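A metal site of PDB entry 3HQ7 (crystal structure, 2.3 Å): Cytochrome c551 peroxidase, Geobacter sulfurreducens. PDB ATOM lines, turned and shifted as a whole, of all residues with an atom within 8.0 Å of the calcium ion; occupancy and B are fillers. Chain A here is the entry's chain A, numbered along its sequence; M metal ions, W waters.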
ATOM      1  N   GLY A  84      -8.458  22.656 -13.713  1.00  0.00           N
ATOM      2  CA  GLY A  84      -7.863  22.096 -14.898  1.00  0.00           C
ATOM      3  C   GLY A  84      -6.340  22.263 -14.703  1.00  0.00           C
ATOM      4  O   GLY A  84      -5.845  22.635 -13.591  1.00  0.00           O
ATOM      5  N   ASP A  85      -5.555  21.960 -15.737  1.00  0.00           N
ATOM      6  CA  ASP A  85      -4.102  22.021 -15.600  1.00  0.00           C
ATOM      7  C   ASP A  85      -3.426  23.126 -16.449  1.00  0.00           C
ATOM      8  O   ASP A  85      -2.195  23.171 -16.577  1.00  0.00           O
ATOM      9  CB  ASP A  85      -3.526  20.650 -15.890  1.00  0.00           C
ATOM     10  CG  ASP A  85      -3.663  20.199 -17.414  1.00  0.00           C
ATOM     11  OD1 ASP A  85      -4.296  20.852 -18.266  1.00  0.00           O
ATOM     12  OD2 ASP A  85      -3.124  19.110 -17.747  1.00  0.00           O
ATOM     13  N   LEU A  86      -4.226  23.996 -17.052  1.00  0.00           N
ATOM     14  CA  LEU A  86      -3.714  24.973 -18.034  1.00  0.00           C
ATOM     15  C   LEU A  86      -2.887  24.506 -19.199  1.00  0.00           C
ATOM     16  O   LEU A  86      -2.125  25.293 -19.813  1.00  0.00           O
ATOM     17  CB  LEU A  86      -2.935  26.099 -17.310  1.00  0.00           C
ATOM     18  CG  LEU A  86      -3.522  26.941 -16.131  1.00  0.00           C
ATOM     19  CD1 LEU A  86      -2.847  28.258 -16.228  1.00  0.00           C
ATOM     20  CD2 LEU A  86      -5.070  27.165 -16.149  1.00  0.00           C
ATOM     21  N   GLN A  87      -2.912  23.224 -19.517  1.00  0.00           N
ATOM     22  CA  GLN A  87      -2.041  22.693 -20.579  1.00  0.00           C
ATOM     23  C   GLN A  87      -2.916  22.359 -21.798  1.00  0.00           C
ATOM     24  O   GLN A  87      -4.143  22.158 -21.646  1.00  0.00           O
ATOM     25  CB  GLN A  87      -1.257  21.488 -20.118  1.00  0.00           C
ATOM     26  CG  GLN A  87      -0.310  21.759 -18.955  1.00  0.00           C
ATOM     27  CD  GLN A  87       0.826  22.696 -19.344  1.00  0.00           C
ATOM     28  OE1 GLN A  87       1.443  22.528 -20.424  1.00  0.00           O
ATOM     29  NE2 GLN A  87       1.112  23.721 -18.500  1.00  0.00           N
ATOM     30  N   ALA A  88      -2.329  22.401 -22.994  1.00  0.00           N
ATOM     31  CA  ALA A  88      -3.005  21.945 -24.218  1.00  0.00           C
ATOM     32  C   ALA A  88      -3.556  20.511 -23.991  1.00  0.00           C
ATOM     33  O   ALA A  88      -4.762  20.280 -24.005  1.00  0.00           O
ATOM     34  CB  ALA A  88      -2.004  21.987 -25.442  1.00  0.00           C
ATOM     35  N   ASN A 101      -7.032  17.065 -23.579  1.00  0.00           N
ATOM     36  CA  ASN A 101      -7.180  18.189 -22.700  1.00  0.00           C
ATOM     37  C   ASN A 101      -7.862  17.797 -21.411  1.00  0.00           C
ATOM     38  O   ASN A 101      -8.974  17.259 -21.403  1.00  0.00           O
ATOM     39  CB  ASN A 101      -8.006  19.310 -23.408  1.00  0.00           C
ATOM     40  CG  ASN A 101      -7.977  20.665 -22.656  1.00  0.00           C
ATOM     41  OD1 ASN A 101      -8.936  21.065 -21.974  1.00  0.00           O
ATOM     42  ND2 ASN A 101      -6.861  21.341 -22.731  1.00  0.00           N
ATOM     43  N   ALA A 102      -7.266  18.202 -20.295  1.00  0.00           N
ATOM     44  CA  ALA A 102      -7.866  17.928 -18.947  1.00  0.00           C
ATOM     45  C   ALA A 102      -9.082  18.744 -18.636  1.00  0.00           C
ATOM     46  O   ALA A 102      -8.976  19.951 -18.540  1.00  0.00           O
ATOM     47  CB  ALA A 102      -6.794  18.001 -17.735  1.00  0.00           C
ATOM     48  N   PRO A 103     -10.261  18.074 -18.456  1.00  0.00           N
ATOM     49  CA  PRO A 103     -11.434  18.907 -18.102  1.00  0.00           C
ATOM     50  C   PRO A 103     -11.396  19.405 -16.708  1.00  0.00           C
ATOM     51  O   PRO A 103     -10.636  18.914 -15.863  1.00  0.00           O
ATOM     52  CB  PRO A 103     -12.636  17.916 -18.258  1.00  0.00           C
ATOM     53  CG  PRO A 103     -12.063  16.508 -18.358  1.00  0.00           C
ATOM     54  CD  PRO A 103     -10.594  16.606 -18.582  1.00  0.00           C
ATOM     55  N   THR A 104     -12.279  20.325 -16.372  1.00  0.00           N
ATOM     56  CA  THR A 104     -12.206  20.849 -15.034  1.00  0.00           C
ATOM     57  C   THR A 104     -12.887  19.835 -14.101  1.00  0.00           C
ATOM     58  O   THR A 104     -13.736  19.045 -14.502  1.00  0.00           O
ATOM     59  CB  THR A 104     -12.802  22.225 -14.954  1.00  0.00           C
ATOM     60  OG1 THR A 104     -12.817  22.639 -13.607  1.00  0.00           O
ATOM     61  CG2 THR A 104     -14.181  22.189 -15.396  1.00  0.00           C
ATOM     62  N   PRO A 270     -18.772  19.652 -24.078  1.00  0.00           N
ATOM     63  CA  PRO A 270     -18.384  20.108 -22.760  1.00  0.00           C
ATOM     64  C   PRO A 270     -19.370  20.907 -21.898  1.00  0.00           C
ATOM     65  O   PRO A 270     -20.191  21.716 -22.353  1.00  0.00           O
ATOM     66  CB  PRO A 270     -17.066  20.814 -23.057  1.00  0.00           C
ATOM     67  CG  PRO A 270     -16.546  20.142 -24.248  1.00  0.00           C
ATOM     68  CD  PRO A 270     -17.708  19.921 -25.077  1.00  0.00           C
ATOM     69  N   VAL A 275     -16.000  28.140 -18.153  1.00  0.00           N
ATOM     70  CA  VAL A 275     -15.083  28.111 -19.386  1.00  0.00           C
ATOM     71  C   VAL A 275     -14.110  29.297 -19.592  1.00  0.00           C
ATOM     72  O   VAL A 275     -13.026  29.233 -20.293  1.00  0.00           O
ATOM     73  CB  VAL A 275     -15.952  27.851 -20.703  1.00  0.00           C
ATOM     74  CG1 VAL A 275     -17.032  28.984 -20.875  1.00  0.00           C
ATOM     75  CG2 VAL A 275     -15.075  27.710 -21.984  1.00  0.00           C
ATOM     76  N   ILE A 277     -12.349  30.473 -17.407  1.00  0.00           N
ATOM     77  CA  ILE A 277     -11.133  30.091 -16.669  1.00  0.00           C
ATOM     78  C   ILE A 277     -10.445  28.731 -17.014  1.00  0.00           C
ATOM     79  O   ILE A 277      -9.414  28.415 -16.427  1.00  0.00           O
ATOM     80  CB  ILE A 277     -11.349  30.343 -15.194  1.00  0.00           C
ATOM     81  CG1 ILE A 277     -12.400  29.455 -14.580  1.00  0.00           C
ATOM     82  CG2 ILE A 277     -11.836  31.813 -14.947  1.00  0.00           C
ATOM     83  CD1 ILE A 277     -12.200  29.481 -13.092  1.00  0.00           C
ATOM     84  N   THR A 278     -10.930  27.946 -17.990  1.00  0.00           N
ATOM     85  CA  THR A 278     -10.357  26.647 -18.274  1.00  0.00           C
ATOM     86  C   THR A 278      -9.711  26.440 -19.700  1.00  0.00           C
ATOM     87  O   THR A 278      -9.732  25.295 -20.255  1.00  0.00           O
ATOM     88  CB  THR A 278     -11.396  25.559 -18.019  1.00  0.00           C
ATOM     89  OG1 THR A 278     -12.444  25.720 -18.993  1.00  0.00           O
ATOM     90  CG2 THR A 278     -11.983  25.663 -16.525  1.00  0.00           C
ATOM     91  N   TYR A 279      -9.192  27.530 -20.269  1.00  0.00           N
ATOM     92  CA  TYR A 279      -8.458  27.526 -21.517  1.00  0.00           C
ATOM     93  C   TYR A 279      -7.340  26.590 -21.325  1.00  0.00           C
ATOM     94  O   TYR A 279      -7.071  26.187 -20.206  1.00  0.00           O
ATOM     95  CB  TYR A 279      -7.912  28.932 -21.832  1.00  0.00           C
ATOM     96  CG  TYR A 279      -7.338  29.537 -20.577  1.00  0.00           C
ATOM     97  CD1 TYR A 279      -5.982  29.350 -20.267  1.00  0.00           C
ATOM     98  CD2 TYR A 279      -8.155  30.224 -19.671  1.00  0.00           C
ATOM     99  CE1 TYR A 279      -5.459  29.822 -19.109  1.00  0.00           C
ATOM    100  CE2 TYR A 279      -7.653  30.700 -18.472  1.00  0.00           C
ATOM    101  CZ  TYR A 279      -6.305  30.452 -18.214  1.00  0.00           C
ATOM    102  OH  TYR A 279      -5.746  30.880 -17.131  1.00  0.00           O
ATOM    103  N   PRO A 280      -6.697  26.118 -22.410  1.00  0.00           N
ATOM    104  CA  PRO A 280      -7.127  26.332 -23.775  1.00  0.00           C
ATOM    105  C   PRO A 280      -8.357  25.489 -24.021  1.00  0.00           C
ATOM    106  O   PRO A 280      -8.822  24.806 -23.089  1.00  0.00           O
ATOM    107  CB  PRO A 280      -5.944  25.865 -24.555  1.00  0.00           C
ATOM    108  CG  PRO A 280      -5.138  24.976 -23.633  1.00  0.00           C
ATOM    109  CD  PRO A 280      -5.502  25.271 -22.276  1.00  0.00           C
ATOM    110  N   TYR A 281      -8.941  25.568 -25.205  1.00  0.00           N
ATOM    111  CA  TYR A 281     -10.259  24.976 -25.497  1.00  0.00           C
ATOM    112  C   TYR A 281     -10.303  23.736 -26.429  1.00  0.00           C
ATOM    113  O   TYR A 281      -9.429  23.514 -27.163  1.00  0.00           O
ATOM    114  CB  TYR A 281     -11.209  26.090 -25.963  1.00  0.00           C
ATOM    115  CG  TYR A 281     -11.253  27.161 -24.897  1.00  0.00           C
ATOM    116  CD1 TYR A 281     -10.498  28.352 -25.046  1.00  0.00           C
ATOM    117  CD2 TYR A 281     -11.961  26.933 -23.715  1.00  0.00           C
ATOM    118  CE1 TYR A 281     -10.490  29.322 -24.028  1.00  0.00           C
ATOM    119  CE2 TYR A 281     -12.014  27.878 -22.734  1.00  0.00           C
ATOM    120  CZ  TYR A 281     -11.274  29.069 -22.896  1.00  0.00           C
ATOM    121  OH  TYR A 281     -11.311  29.982 -21.903  1.00  0.00           O
ATOM    122  N   PHE A 282     -11.368  22.938 -26.372  1.00  0.00           N
ATOM    123  CA  PHE A 282     -11.455  21.706 -27.223  1.00  0.00           C
ATOM    124  C   PHE A 282     -10.527  20.580 -26.838  1.00  0.00           C
ATOM    125  O   PHE A 282      -9.391  20.846 -26.430  1.00  0.00           O
ATOM    126  CB  PHE A 282     -11.284  21.965 -28.759  1.00  0.00           C
ATOM    127  CG  PHE A 282     -12.124  23.070 -29.248  1.00  0.00           C
ATOM    128  CD1 PHE A 282     -11.537  24.203 -29.835  1.00  0.00           C
ATOM    129  CD2 PHE A 282     -13.501  23.042 -29.009  1.00  0.00           C
ATOM    130  CE1 PHE A 282     -12.312  25.268 -30.248  1.00  0.00           C
ATOM    131  CE2 PHE A 282     -14.319  24.137 -29.415  1.00  0.00           C
ATOM    132  CZ  PHE A 282     -13.726  25.241 -30.041  1.00  0.00           C
ATOM    133  N   HIS A 283     -11.018  19.369 -27.052  1.00  0.00           N
ATOM    134  CA  HIS A 283     -10.373  18.083 -26.721  1.00  0.00           C
ATOM    135  C   HIS A 283      -8.818  18.106 -26.909  1.00  0.00           C
ATOM    136  O   HIS A 283      -8.109  17.318 -26.258  1.00  0.00           O
ATOM    137  CB  HIS A 283     -11.055  16.932 -27.530  1.00  0.00           C
ATOM    138  CG  HIS A 283     -10.548  16.838 -28.945  1.00  0.00           C
ATOM    139  ND1 HIS A 283     -11.149  17.498 -30.006  1.00  0.00           N
ATOM    140  CD2 HIS A 283      -9.418  16.264 -29.445  1.00  0.00           C
ATOM    141  CE1 HIS A 283     -10.460  17.269 -31.111  1.00  0.00           C
ATOM    142  NE2 HIS A 283      -9.391  16.550 -30.794  1.00  0.00           N
ATOM    143  N   SER A 284      -8.285  19.002 -27.747  1.00  0.00           N
ATOM    144  CA  SER A 284      -6.897  18.996 -28.078  1.00  0.00           C
ATOM    145  C   SER A 284      -6.278  20.300 -27.611  1.00  0.00           C
ATOM    146  O   SER A 284      -5.099  20.583 -27.860  1.00  0.00           O
ATOM    147  CB  SER A 284      -6.732  18.872 -29.630  1.00  0.00           C
ATOM    148  OG  SER A 284      -7.470  19.906 -30.336  1.00  0.00           O
ATOM    149  N   GLY A 285      -7.072  21.129 -26.978  1.00  0.00           N
ATOM    150  CA  GLY A 285      -6.532  22.296 -26.296  1.00  0.00           C
ATOM    151  C   GLY A 285      -5.802  23.203 -27.227  1.00  0.00           C
ATOM    152  O   GLY A 285      -4.717  23.690 -26.878  1.00  0.00           O
ATOM    153  N   VAL A 286      -6.376  23.470 -28.421  1.00  0.00           N
ATOM    154  CA  VAL A 286      -5.583  24.188 -29.493  1.00  0.00           C
ATOM    155  C   VAL A 286      -5.979  25.652 -29.650  1.00  0.00           C
ATOM    156  O   VAL A 286      -5.208  26.448 -30.182  1.00  0.00           O
ATOM    157  CB  VAL A 286      -5.677  23.497 -30.933  1.00  0.00           C
ATOM    158  CG1 VAL A 286      -4.509  22.510 -31.174  1.00  0.00           C
ATOM    159  CG2 VAL A 286      -7.104  22.968 -31.202  1.00  0.00           C
ATOM    160  N   VAL A 287      -7.209  25.964 -29.284  1.00  0.00           N
ATOM    161  CA  VAL A 287      -7.674  27.359 -29.266  1.00  0.00           C
ATOM    162  C   VAL A 287      -7.423  28.034 -27.828  1.00  0.00           C
ATOM    163  O   VAL A 287      -7.986  27.605 -26.822  1.00  0.00           O
ATOM    164  CB  VAL A 287      -9.158  27.473 -29.861  1.00  0.00           C
ATOM    165  CG1 VAL A 287      -9.872  28.840 -29.563  1.00  0.00           C
ATOM    166  CG2 VAL A 287      -9.162  27.246 -31.384  1.00  0.00           C
HETATM  167 CA    CA M   1      -9.786  23.213 -21.424  1.00  0.00          CA
HETATM  168  O   HOH W   1     -10.575  22.443 -20.108  1.00  0.00           O
HETATM  169  O   HOH W   2     -11.632  24.265 -21.120  1.00  0.00           O
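ND2 of Asn 101 is in hydrogen-bond range of O of Gln 87, 3.0 Å away.
ND2 of Asn 101 is in hydrogen-bond range of O of Ala 88 (2.7 Å).
O of His 283 is in hydrogen-bond range of N of Asn 101, 2.9 Å away.
Within 4 Å of the calcium ion: Asn 101, Thr 278 and Pro 280.
The nearest printed residue that does not touch the calcium ion is Tyr 279 (4.2 Å).
The calcium ion is bound by water W1 (1.7 Å), water W2 (2.1 Å), the side-chain amide oxygen (OD1) of Asn 101 (2.4 Å), the backbone carbonyl oxygen (O) of Thr 278 (2.4 Å) and the backbone carbonyl oxygen (O) of Pro 280 (2.5 Å).
The calcium ion has five donor atoms within binding distance.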
